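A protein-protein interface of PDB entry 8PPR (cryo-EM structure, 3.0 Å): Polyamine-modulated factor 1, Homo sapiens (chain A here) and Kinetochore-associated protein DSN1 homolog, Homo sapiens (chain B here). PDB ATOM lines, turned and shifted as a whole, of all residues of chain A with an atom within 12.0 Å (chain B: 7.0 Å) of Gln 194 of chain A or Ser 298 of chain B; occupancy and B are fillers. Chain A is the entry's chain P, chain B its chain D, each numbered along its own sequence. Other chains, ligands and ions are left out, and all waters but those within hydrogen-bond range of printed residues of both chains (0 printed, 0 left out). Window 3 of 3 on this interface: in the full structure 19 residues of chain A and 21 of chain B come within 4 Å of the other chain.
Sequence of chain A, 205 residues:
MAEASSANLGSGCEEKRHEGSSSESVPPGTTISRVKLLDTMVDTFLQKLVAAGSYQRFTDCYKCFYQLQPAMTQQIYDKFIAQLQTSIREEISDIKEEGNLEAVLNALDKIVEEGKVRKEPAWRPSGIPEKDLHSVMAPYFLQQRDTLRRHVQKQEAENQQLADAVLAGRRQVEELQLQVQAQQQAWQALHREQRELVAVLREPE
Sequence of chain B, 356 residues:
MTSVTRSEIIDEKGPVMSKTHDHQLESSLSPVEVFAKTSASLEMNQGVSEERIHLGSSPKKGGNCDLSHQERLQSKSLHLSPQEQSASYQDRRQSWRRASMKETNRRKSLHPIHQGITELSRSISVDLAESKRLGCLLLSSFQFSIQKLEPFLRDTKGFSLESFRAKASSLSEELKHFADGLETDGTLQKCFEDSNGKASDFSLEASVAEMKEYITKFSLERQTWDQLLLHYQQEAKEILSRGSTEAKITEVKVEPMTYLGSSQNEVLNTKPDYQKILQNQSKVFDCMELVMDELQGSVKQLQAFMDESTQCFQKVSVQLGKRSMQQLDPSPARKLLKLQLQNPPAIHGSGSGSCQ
The side-chain amide oxygen (OE1) of Gln 194 of chain A sits close to the side-chain carboxylate (OE2) of Glu 294 of chain B. The side-chain carboxylate (OE2) of Glu 294 of chain B sits at hydrogen-bond distance from a ring nitrogen (ND1) of His 191 of chain A (3.2 Å). NE2 of Gln 194 of chain A lies close to N of Leu 295 of chain B (3.4 Å).
The side-chain amide oxygen (OE1) of Gln 194 of chain A lies close to the backbone carbonyl oxygen (O) of Leu 190 of chain A (3.5 Å).
Among the printed residues, merely in contact across the chains: Gln 194 of chain A with Ser 298 of chain B (3.5 Å), Trp 187 of chain A with Val 291 of chain B (3.8 Å), Leu 190 of chain A with Leu 295 of chain B (3.8 Å) and Gln 188 of chain A with Val 291 of chain B (3.99 Å).
Gln 194 of chain A touches three residues of chain B. Of the printed residues of chain A, Ser 298 of chain B touches Gln 194 (3.5 Å). Of chain A, only His 191 (3.2 Å) and Gln 194 (2.9 Å) come within 4 Å of Glu 294 of chain B. Leu 295 of chain B touches just these residues of chain A: Leu 190 and Gln 194. Gly 297 of chain B touches none of the printed residues of chain A. No residue of chain A comes within 4 Å of Val 299 of chain B. No residue of chain A comes within 4 Å of Lys 300 of chain B. Of the printed residues of chain A, Val 291 of chain B touches Trp 187 and Gln 188. Printed residues of chain B within 4 Å of His 191 of chain A: Glu 294 (3.2 Å). Of the printed residues of chain B, Leu 190 of chain A touches Leu 295 (3.8 Å). Met 292 of chain B touches none of the printed residues of chain A. The nearest residue of chain B that does not touch Gln 194 of chain A is Val 291 of chain B (4.5 Å). The nearest residue of chain A that does not touch Ser 298 of chain B is Leu 197 of chain A (4.8 Å).
Printed residues of chain B that touch a printed residue of chain A: Val 291, Glu 294, Leu 295 and Ser 298. Hydrophobic or aromatic side chains of chain B within 4 Å of the printed part of chain A: Val 291 and Leu 295. Along chain B the printed residues that touch a printed residue of chain A span positions 291 to 298. Of the 20 printed residues of chain A, 5 touch a printed residue of chain B. Hydrophobic or aromatic side chains of chain A within 4 Å of the printed part of chain B: Leu 190 and His 191. Along chain A the printed residues that touch a printed residue of chain B span positions 187 to 194.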
ATOM      1  N   GLN A 184      21.227  25.407   7.840  1.00  0.00           N
ATOM      2  CA  GLN A 184      19.953  25.407   7.133  1.00  0.00           C
ATOM      3  C   GLN A 184      20.127  24.982   5.683  1.00  0.00           C
ATOM      4  O   GLN A 184      19.365  24.154   5.174  1.00  0.00           O
ATOM      5  CB  GLN A 184      19.325  26.797   7.207  1.00  0.00           C
ATOM      6  CG  GLN A 184      17.983  26.922   6.518  1.00  0.00           C
ATOM      7  CD  GLN A 184      17.438  28.333   6.581  1.00  0.00           C
ATOM      8  OE1 GLN A 184      16.348  28.614   6.087  1.00  0.00           O
ATOM      9  NE2 GLN A 184      18.200  29.232   7.193  1.00  0.00           N
ATOM     10  N   GLN A 185      21.136  25.530   5.008  1.00  0.00           N
ATOM     11  CA  GLN A 185      21.368  25.186   3.611  1.00  0.00           C
ATOM     12  C   GLN A 185      21.814  23.741   3.458  1.00  0.00           C
ATOM     13  O   GLN A 185      21.419  23.067   2.498  1.00  0.00           O
ATOM     14  CB  GLN A 185      22.404  26.134   3.016  1.00  0.00           C
ATOM     15  CG  GLN A 185      21.811  27.429   2.499  1.00  0.00           C
ATOM     16  CD  GLN A 185      22.868  28.397   2.017  1.00  0.00           C
ATOM     17  OE1 GLN A 185      24.060  28.194   2.241  1.00  0.00           O
ATOM     18  NE2 GLN A 185      22.434  29.463   1.354  1.00  0.00           N
ATOM     19  N   ALA A 186      22.628  23.246   4.392  1.00  0.00           N
ATOM     20  CA  ALA A 186      23.037  21.849   4.347  1.00  0.00           C
ATOM     21  C   ALA A 186      21.834  20.929   4.475  1.00  0.00           C
ATOM     22  O   ALA A 186      21.741  19.913   3.776  1.00  0.00           O
ATOM     23  CB  ALA A 186      24.054  21.563   5.452  1.00  0.00           C
ATOM     24  N   TRP A 187      20.896  21.270   5.358  1.00  0.00           N
ATOM     25  CA  TRP A 187      19.697  20.453   5.482  1.00  0.00           C
ATOM     26  C   TRP A 187      18.753  20.621   4.299  1.00  0.00           C
ATOM     27  O   TRP A 187      18.022  19.682   3.968  1.00  0.00           O
ATOM     28  CB  TRP A 187      18.968  20.775   6.782  1.00  0.00           C
ATOM     29  CG  TRP A 187      19.406  19.905   7.906  1.00  0.00           C
ATOM     30  CD1 TRP A 187      20.226  20.249   8.938  1.00  0.00           C
ATOM     31  CD2 TRP A 187      19.083  18.525   8.091  1.00  0.00           C
ATOM     32  NE1 TRP A 187      20.415  19.172   9.770  1.00  0.00           N
ATOM     33  CE2 TRP A 187      19.725  18.099   9.270  1.00  0.00           C
ATOM     34  CE3 TRP A 187      18.305  17.608   7.379  1.00  0.00           C
ATOM     35  CZ2 TRP A 187      19.613  16.799   9.753  1.00  0.00           C
ATOM     36  CZ3 TRP A 187      18.194  16.317   7.859  1.00  0.00           C
ATOM     37  CH2 TRP A 187      18.845  15.925   9.035  1.00  0.00           C
ATOM     38  N   GLN A 188      18.757  21.783   3.654  1.00  0.00           N
ATOM     39  CA  GLN A 188      17.878  22.034   2.520  1.00  0.00           C
ATOM     40  C   GLN A 188      18.431  21.502   1.207  1.00  0.00           C
ATOM     41  O   GLN A 188      17.692  21.443   0.219  1.00  0.00           O
ATOM     42  CB  GLN A 188      17.612  23.536   2.387  1.00  0.00           C
ATOM     43  CG  GLN A 188      16.711  24.101   3.469  1.00  0.00           C
ATOM     44  CD  GLN A 188      15.979  25.348   3.022  1.00  0.00           C
ATOM     45  OE1 GLN A 188      16.440  26.067   2.136  1.00  0.00           O
ATOM     46  NE2 GLN A 188      14.833  25.615   3.636  1.00  0.00           N
ATOM     47  N   ALA A 189      19.706  21.114   1.175  1.00  0.00           N
ATOM     48  CA  ALA A 189      20.294  20.566  -0.041  1.00  0.00           C
ATOM     49  C   ALA A 189      19.685  19.231  -0.453  1.00  0.00           C
ATOM     50  O   ALA A 189      19.923  18.785  -1.580  1.00  0.00           O
ATOM     51  CB  ALA A 189      21.804  20.408   0.134  1.00  0.00           C
ATOM     52  N   LEU A 190      18.910  18.586   0.420  1.00  0.00           N
ATOM     53  CA  LEU A 190      18.281  17.312   0.090  1.00  0.00           C
ATOM     54  C   LEU A 190      17.208  17.445  -0.981  1.00  0.00           C
ATOM     55  O   LEU A 190      16.740  16.422  -1.499  1.00  0.00           O
ATOM     56  CB  LEU A 190      17.667  16.700   1.349  1.00  0.00           C
ATOM     57  CG  LEU A 190      18.548  16.647   2.599  1.00  0.00           C
ATOM     58  CD1 LEU A 190      17.814  15.972   3.747  1.00  0.00           C
ATOM     59  CD2 LEU A 190      19.853  15.930   2.307  1.00  0.00           C
ATOM     60  N   HIS A 191      16.804  18.674  -1.311  1.00  0.00           N
ATOM     61  CA  HIS A 191      15.692  18.883  -2.231  1.00  0.00           C
ATOM     62  C   HIS A 191      16.002  18.350  -3.621  1.00  0.00           C
ATOM     63  O   HIS A 191      15.128  17.772  -4.277  1.00  0.00           O
ATOM     64  CB  HIS A 191      15.345  20.369  -2.294  1.00  0.00           C
ATOM     65  CG  HIS A 191      14.398  20.723  -3.398  1.00  0.00           C
ATOM     66  ND1 HIS A 191      13.030  20.720  -3.234  1.00  0.00           N
ATOM     67  CD2 HIS A 191      14.623  21.104  -4.678  1.00  0.00           C
ATOM     68  CE1 HIS A 191      12.453  21.078  -4.367  1.00  0.00           C
ATOM     69  NE2 HIS A 191      13.396  21.315  -5.260  1.00  0.00           N
ATOM     70  N   ARG A 192      17.228  18.561  -4.103  1.00  0.00           N
ATOM     71  CA  ARG A 192      17.572  18.094  -5.442  1.00  0.00           C
ATOM     72  C   ARG A 192      17.473  16.578  -5.535  1.00  0.00           C
ATOM     73  O   ARG A 192      16.906  16.041  -6.492  1.00  0.00           O
ATOM     74  CB  ARG A 192      18.974  18.564  -5.820  1.00  0.00           C
ATOM     75  CG  ARG A 192      19.368  18.213  -7.241  1.00  0.00           C
ATOM     76  CD  ARG A 192      20.870  18.278  -7.432  1.00  0.00           C
ATOM     77  NE  ARG A 192      21.345  19.649  -7.567  1.00  0.00           N
ATOM     78  CZ  ARG A 192      21.579  20.248  -8.727  1.00  0.00           C
ATOM     79  NH1 ARG A 192      21.356  19.636  -9.878  1.00  0.00           N
ATOM     80  NH2 ARG A 192      22.046  21.494  -8.731  1.00  0.00           N
ATOM     81  N   GLU A 193      18.010  15.872  -4.537  1.00  0.00           N
ATOM     82  CA  GLU A 193      17.914  14.418  -4.528  1.00  0.00           C
ATOM     83  C   GLU A 193      16.468  13.961  -4.408  1.00  0.00           C
ATOM     84  O   GLU A 193      16.064  12.983  -5.047  1.00  0.00           O
ATOM     85  CB  GLU A 193      18.755  13.843  -3.388  1.00  0.00           C
ATOM     86  CG  GLU A 193      20.015  14.635  -3.078  1.00  0.00           C
ATOM     87  CD  GLU A 193      21.083  14.514  -4.152  1.00  0.00           C
ATOM     88  OE1 GLU A 193      20.860  13.801  -5.155  1.00  0.00           O
ATOM     89  OE2 GLU A 193      22.151  15.138  -3.993  1.00  0.00           O
ATOM     90  N   GLN A 194      15.673  14.649  -3.586  1.00  0.00           N
ATOM     91  CA  GLN A 194      14.274  14.265  -3.437  1.00  0.00           C
ATOM     92  C   GLN A 194      13.511  14.424  -4.746  1.00  0.00           C
ATOM     93  O   GLN A 194      12.736  13.542  -5.134  1.00  0.00           O
ATOM     94  CB  GLN A 194      13.624  15.090  -2.330  1.00  0.00           C
ATOM     95  CG  GLN A 194      13.903  14.567  -0.937  1.00  0.00           C
ATOM     96  CD  GLN A 194      13.656  15.607   0.132  1.00  0.00           C
ATOM     97  OE1 GLN A 194      13.584  16.801  -0.154  1.00  0.00           O
ATOM     98  NE2 GLN A 194      13.513  15.157   1.371  1.00  0.00           N
ATOM     99  N   ARG A 195      13.731  15.535  -5.450  1.00  0.00           N
ATOM    100  CA  ARG A 195      13.060  15.730  -6.729  1.00  0.00           C
ATOM    101  C   ARG A 195      13.563  14.747  -7.774  1.00  0.00           C
ATOM    102  O   ARG A 195      12.783  14.284  -8.612  1.00  0.00           O
ATOM    103  CB  ARG A 195      13.244  17.168  -7.211  1.00  0.00           C
ATOM    104  CG  ARG A 195      12.707  18.207  -6.245  1.00  0.00           C
ATOM    105  CD  ARG A 195      11.251  17.946  -5.895  1.00  0.00           C
ATOM    106  NE  ARG A 195      10.378  18.006  -7.062  1.00  0.00           N
ATOM    107  CZ  ARG A 195       9.130  17.560  -7.085  1.00  0.00           C
ATOM    108  NH1 ARG A 195       8.573  17.007  -6.020  1.00  0.00           N
ATOM    109  NH2 ARG A 195       8.421  17.674  -8.204  1.00  0.00           N
ATOM    110  N   GLU A 196      14.852  14.407  -7.737  1.00  0.00           N
ATOM    111  CA  GLU A 196      15.365  13.385  -8.641  1.00  0.00           C
ATOM    112  C   GLU A 196      14.697  12.042  -8.382  1.00  0.00           C
ATOM    113  O   GLU A 196      14.340  11.324  -9.323  1.00  0.00           O
ATOM    114  CB  GLU A 196      16.881  13.269  -8.494  1.00  0.00           C
ATOM    115  CG  GLU A 196      17.506  12.242  -9.416  1.00  0.00           C
ATOM    116  CD  GLU A 196      17.290  12.567 -10.880  1.00  0.00           C
ATOM    117  OE1 GLU A 196      17.188  13.765 -11.220  1.00  0.00           O
ATOM    118  OE2 GLU A 196      17.217  11.622 -11.693  1.00  0.00           O
ATOM    119  N   LEU A 197      14.523  11.687  -7.109  1.00  0.00           N
ATOM    120  CA  LEU A 197      13.835  10.447  -6.774  1.00  0.00           C
ATOM    121  C   LEU A 197      12.391  10.477  -7.254  1.00  0.00           C
ATOM    122  O   LEU A 197      11.880   9.479  -7.777  1.00  0.00           O
ATOM    123  CB  LEU A 197      13.892  10.208  -5.267  1.00  0.00           C
ATOM    124  CG  LEU A 197      13.264   8.904  -4.777  1.00  0.00           C
ATOM    125  CD1 LEU A 197      13.748   7.733  -5.616  1.00  0.00           C
ATOM    126  CD2 LEU A 197      13.584   8.683  -3.308  1.00  0.00           C
ATOM    127  N   VAL A 198      11.717  11.615  -7.079  1.00  0.00           N
ATOM    128  CA  VAL A 198      10.349  11.752  -7.570  1.00  0.00           C
ATOM    129  C   VAL A 198      10.309  11.556  -9.079  1.00  0.00           C
ATOM    130  O   VAL A 198       9.398  10.915  -9.616  1.00  0.00           O
ATOM    131  CB  VAL A 198       9.769  13.116  -7.157  1.00  0.00           C
ATOM    132  CG1 VAL A 198       8.456  13.379  -7.875  1.00  0.00           C
ATOM    133  CG2 VAL A 198       9.575  13.172  -5.652  1.00  0.00           C
ATOM    134  N   ALA A 199      11.302  12.098  -9.784  1.00  0.00           N
ATOM    135  CA  ALA A 199      11.384  11.894 -11.226  1.00  0.00           C
ATOM    136  C   ALA A 199      11.586  10.423 -11.561  1.00  0.00           C
ATOM    137  O   ALA A 199      10.994   9.908 -12.517  1.00  0.00           O
ATOM    138  CB  ALA A 199      12.514  12.739 -11.812  1.00  0.00           C
ATOM    139  N   VAL A 200      12.421   9.731 -10.786  1.00  0.00           N
ATOM    140  CA  VAL A 200      12.644   8.307 -11.016  1.00  0.00           C
ATOM    141  C   VAL A 200      11.355   7.527 -10.798  1.00  0.00           C
ATOM    142  O   VAL A 200      10.971   6.685 -11.617  1.00  0.00           O
ATOM    143  CB  VAL A 200      13.774   7.789 -10.110  1.00  0.00           C
ATOM    144  CG1 VAL A 200      13.853   6.272 -10.174  1.00  0.00           C
ATOM    145  CG2 VAL A 200      15.100   8.412 -10.509  1.00  0.00           C
ATOM    146  N   LEU A 201      10.661   7.806  -9.697  1.00  0.00           N
ATOM    147  CA  LEU A 201       9.401   7.140  -9.379  1.00  0.00           C
ATOM    148  C   LEU A 201       8.267   8.047  -9.843  1.00  0.00           C
ATOM    149  O   LEU A 201       7.639   8.763  -9.064  1.00  0.00           O
ATOM    150  CB  LEU A 201       9.315   6.832  -7.890  1.00  0.00           C
ATOM    151  CG  LEU A 201      10.587   6.250  -7.275  1.00  0.00           C
ATOM    152  CD1 LEU A 201      10.416   6.054  -5.778  1.00  0.00           C
ATOM    153  CD2 LEU A 201      10.961   4.941  -7.954  1.00  0.00           C
ATOM    154  N   ARG A 202       8.005   8.004 -11.141  1.00  0.00           N
ATOM    155  CA  ARG A 202       7.019   8.867 -11.765  1.00  0.00           C
ATOM    156  C   ARG A 202       5.656   8.188 -11.810  1.00  0.00           C
ATOM    157  O   ARG A 202       5.538   6.962 -11.753  1.00  0.00           O
ATOM    158  CB  ARG A 202       7.460   9.247 -13.178  1.00  0.00           C
ATOM    159  CG  ARG A 202       7.378   8.099 -14.157  1.00  0.00           C
ATOM    160  CD  ARG A 202       8.295   8.329 -15.339  1.00  0.00           C
ATOM    161  NE  ARG A 202       9.629   7.802 -15.077  1.00  0.00           N
ATOM    162  CZ  ARG A 202       9.938   6.513 -15.052  1.00  0.00           C
ATOM    163  NH1 ARG A 202       9.031   5.578 -15.285  1.00  0.00           N
ATOM    164  NH2 ARG A 202      11.190   6.151 -14.785  1.00  0.00           N
ATOM    165  N   GLU A 203       4.622   9.015 -11.911  1.00  0.00           N
ATOM    166  CA  GLU A 203       3.263   8.522 -11.995  1.00  0.00           C
ATOM    167  C   GLU A 203       3.030   7.851 -13.345  1.00  0.00           C
ATOM    168  O   GLU A 203       3.724   8.144 -14.323  1.00  0.00           O
ATOM    169  CB  GLU A 203       2.283   9.674 -11.788  1.00  0.00           C
ATOM    170  CG  GLU A 203       2.634  10.555 -10.599  1.00  0.00           C
ATOM    171  CD  GLU A 203       1.580  11.604 -10.311  1.00  0.00           C
ATOM    172  OE1 GLU A 203       0.484  11.525 -10.900  1.00  0.00           O
ATOM    173  OE2 GLU A 203       1.848  12.506  -9.489  1.00  0.00           O
ATOM    174  N   VAL B 291      11.099  20.822   5.476  1.00  0.00           N
ATOM    175  CA  VAL B 291      12.019  19.841   4.909  1.00  0.00           C
ATOM    176  C   VAL B 291      11.737  18.467   5.490  1.00  0.00           C
ATOM    177  O   VAL B 291      11.816  17.444   4.796  1.00  0.00           O
ATOM    178  CB  VAL B 291      13.477  20.271   5.161  1.00  0.00           C
ATOM    179  CG1 VAL B 291      14.429  19.110   4.911  1.00  0.00           C
ATOM    180  CG2 VAL B 291      13.835  21.463   4.290  1.00  0.00           C
ATOM    181  N   MET B 292      11.402  18.423   6.776  1.00  0.00           N
ATOM    182  CA  MET B 292      11.094  17.157   7.421  1.00  0.00           C
ATOM    183  C   MET B 292       9.858  16.515   6.806  1.00  0.00           C
ATOM    184  O   MET B 292       9.816  15.295   6.586  1.00  0.00           O
ATOM    185  CB  MET B 292      10.889  17.391   8.913  1.00  0.00           C
ATOM    186  CG  MET B 292      10.741  16.112   9.631  1.00  0.00           C
ATOM    187  SD  MET B 292      12.346  15.344   9.440  1.00  0.00           S
ATOM    188  CE  MET B 292      11.868  13.661   9.645  1.00  0.00           C
ATOM    189  N   ASP B 293       8.836  17.324   6.529  1.00  0.00           N
ATOM    190  CA  ASP B 293       7.642  16.811   5.864  1.00  0.00           C
ATOM    191  C   ASP B 293       7.989  16.256   4.491  1.00  0.00           C
ATOM    192  O   ASP B 293       7.493  15.194   4.090  1.00  0.00           O
ATOM    193  CB  ASP B 293       6.592  17.914   5.745  1.00  0.00           C
ATOM    194  CG  ASP B 293       6.175  18.466   7.084  1.00  0.00           C
ATOM    195  OD1 ASP B 293       6.615  17.917   8.116  1.00  0.00           O
ATOM    196  OD2 ASP B 293       5.427  19.465   7.103  1.00  0.00           O
ATOM    197  N   GLU B 294       8.839  16.974   3.753  1.00  0.00           N
ATOM    198  CA  GLU B 294       9.266  16.497   2.441  1.00  0.00           C
ATOM    199  C   GLU B 294       9.976  15.153   2.547  1.00  0.00           C
ATOM    200  O   GLU B 294       9.747  14.248   1.731  1.00  0.00           O
ATOM    201  CB  GLU B 294      10.182  17.530   1.784  1.00  0.00           C
ATOM    202  CG  GLU B 294      10.417  17.301   0.301  1.00  0.00           C
ATOM    203  CD  GLU B 294      10.736  18.584  -0.443  1.00  0.00           C
ATOM    204  OE1 GLU B 294      10.135  19.628  -0.114  1.00  0.00           O
ATOM    205  OE2 GLU B 294      11.587  18.549  -1.358  1.00  0.00           O
ATOM    206  N   LEU B 295      10.849  15.009   3.545  1.00  0.00           N
ATOM    207  CA  LEU B 295      11.560  13.751   3.744  1.00  0.00           C
ATOM    208  C   LEU B 295      10.592  12.614   4.035  1.00  0.00           C
ATOM    209  O   LEU B 295      10.725  11.511   3.485  1.00  0.00           O
ATOM    210  CB  LEU B 295      12.561  13.898   4.887  1.00  0.00           C
ATOM    211  CG  LEU B 295      13.990  14.278   4.512  1.00  0.00           C
ATOM    212  CD1 LEU B 295      14.737  14.810   5.725  1.00  0.00           C
ATOM    213  CD2 LEU B 295      14.714  13.090   3.904  1.00  0.00           C
ATOM    214  N   GLN B 296       9.613  12.866   4.906  1.00  0.00           N
ATOM    215  CA  GLN B 296       8.631  11.836   5.225  1.00  0.00           C
ATOM    216  C   GLN B 296       7.852  11.421   3.984  1.00  0.00           C
ATOM    217  O   GLN B 296       7.616  10.227   3.757  1.00  0.00           O
ATOM    218  CB  GLN B 296       7.682  12.337   6.310  1.00  0.00           C
ATOM    219  CG  GLN B 296       8.151  12.032   7.715  1.00  0.00           C
ATOM    220  CD  GLN B 296       7.028  12.055   8.724  1.00  0.00           C
ATOM    221  OE1 GLN B 296       5.929  12.531   8.438  1.00  0.00           O
ATOM    222  NE2 GLN B 296       7.297  11.543   9.919  1.00  0.00           N
ATOM    223  N   GLY B 297       7.445  12.396   3.171  1.00  0.00           N
ATOM    224  CA  GLY B 297       6.729  12.071   1.947  1.00  0.00           C
ATOM    225  C   GLY B 297       7.560  11.241   0.989  1.00  0.00           C
ATOM    226  O   GLY B 297       7.061  10.291   0.376  1.00  0.00           O
ATOM    227  N   SER B 298       8.840  11.589   0.844  1.00  0.00           N
ATOM    228  CA  SER B 298       9.711  10.817  -0.037  1.00  0.00           C
ATOM    229  C   SER B 298       9.857   9.383   0.455  1.00  0.00           C
ATOM    230  O   SER B 298       9.814   8.434  -0.341  1.00  0.00           O
ATOM    231  CB  SER B 298      11.075  11.495  -0.143  1.00  0.00           C
ATOM    232  OG  SER B 298      11.035  12.568  -1.067  1.00  0.00           O
ATOM    233  N   VAL B 299      10.022   9.206   1.768  1.00  0.00           N
ATOM    234  CA  VAL B 299      10.154   7.860   2.319  1.00  0.00           C
ATOM    235  C   VAL B 299       8.881   7.060   2.080  1.00  0.00           C
ATOM    236  O   VAL B 299       8.931   5.874   1.727  1.00  0.00           O
ATOM    237  CB  VAL B 299      10.508   7.929   3.816  1.00  0.00           C
ATOM    238  CG1 VAL B 299      10.405   6.551   4.450  1.00  0.00           C
ATOM    239  CG2 VAL B 299      11.903   8.503   4.000  1.00  0.00           C
ATOM    240  N   LYS B 300       7.721   7.691   2.271  1.00  0.00           N
ATOM    241  CA  LYS B 300       6.458   6.997   2.039  1.00  0.00           C
ATOM    242  C   LYS B 300       6.323   6.568   0.584  1.00  0.00           C
ATOM    243  O   LYS B 300       5.884   5.444   0.292  1.00  0.00           O
ATOM    244  CB  LYS B 300       5.290   7.898   2.433  1.00  0.00           C
ATOM    245  CG  LYS B 300       3.936   7.382   1.996  1.00  0.00           C
ATOM    246  CD  LYS B 300       3.109   8.506   1.405  1.00  0.00           C
ATOM    247  CE  LYS B 300       2.563   9.426   2.482  1.00  0.00           C
ATOM    248  NZ  LYS B 300       1.557  10.375   1.931  1.00  0.00           N
ATOM    249  N   GLN B 301       6.684   7.457  -0.346  1.00  0.00           N
ATOM    250  CA  GLN B 301       6.612   7.104  -1.760  1.00  0.00           C
ATOM    251  C   GLN B 301       7.527   5.930  -2.084  1.00  0.00           C
ATOM    252  O   GLN B 301       7.123   4.996  -2.786  1.00  0.00           O
ATOM    253  CB  GLN B 301       6.957   8.314  -2.623  1.00  0.00           C
ATOM    254  CG  GLN B 301       5.872   9.374  -2.640  1.00  0.00           C
ATOM    255  CD  GLN B 301       4.558   8.858  -3.205  1.00  0.00           C
ATOM    256  OE1 GLN B 301       4.354   8.860  -4.422  1.00  0.00           O
ATOM    257  NE2 GLN B 301       3.671   8.398  -2.333  1.00  0.00           N
ATOM    258  N   LEU B 302       8.756   5.945  -1.559  1.00  0.00           N
ATOM    259  CA  LEU B 302       9.673   4.838  -1.815  1.00  0.00           C
ATOM    260  C   LEU B 302       9.136   3.529  -1.247  1.00  0.00           C
ATOM    261  O   LEU B 302       9.249   2.469  -1.880  1.00  0.00           O
ATOM    262  CB  LEU B 302      11.045   5.149  -1.226  1.00  0.00           C
ATOM    263  CG  LEU B 302      12.112   4.086  -1.497  1.00  0.00           C
ATOM    264  CD1 LEU B 302      12.318   3.903  -2.993  1.00  0.00           C
ATOM    265  CD2 LEU B 302      13.415   4.436  -0.798  1.00  0.00           C
ATOM    266  N   GLN B 303       8.560   3.582  -0.046  1.00  0.00           N
ATOM    267  CA  GLN B 303       7.995   2.384   0.563  1.00  0.00           C
ATOM    268  C   GLN B 303       6.886   1.804  -0.297  1.00  0.00           C
ATOM    269  O   GLN B 303       6.895   0.605  -0.617  1.00  0.00           O
ATOM    270  CB  GLN B 303       7.491   2.689   1.981  1.00  0.00           C
ATOM    271  CG  GLN B 303       8.567   2.490   3.039  1.00  0.00           C
ATOM    272  CD  GLN B 303       8.276   3.208   4.345  1.00  0.00           C
ATOM    273  OE1 GLN B 303       7.207   3.798   4.519  1.00  0.00           O
ATOM    274  NE2 GLN B 303       9.222   3.151   5.275  1.00  0.00           N
ATOM    275  N   ALA B 304       5.946   2.650  -0.719  1.00  0.00           N
ATOM    276  CA  ALA B 304       4.894   2.172  -1.604  1.00  0.00           C
ATOM    277  C   ALA B 304       5.484   1.614  -2.887  1.00  0.00           C
ATOM    278  O   ALA B 304       4.969   0.635  -3.446  1.00  0.00           O
ATOM    279  CB  ALA B 304       3.909   3.296  -1.905  1.00  0.00           C
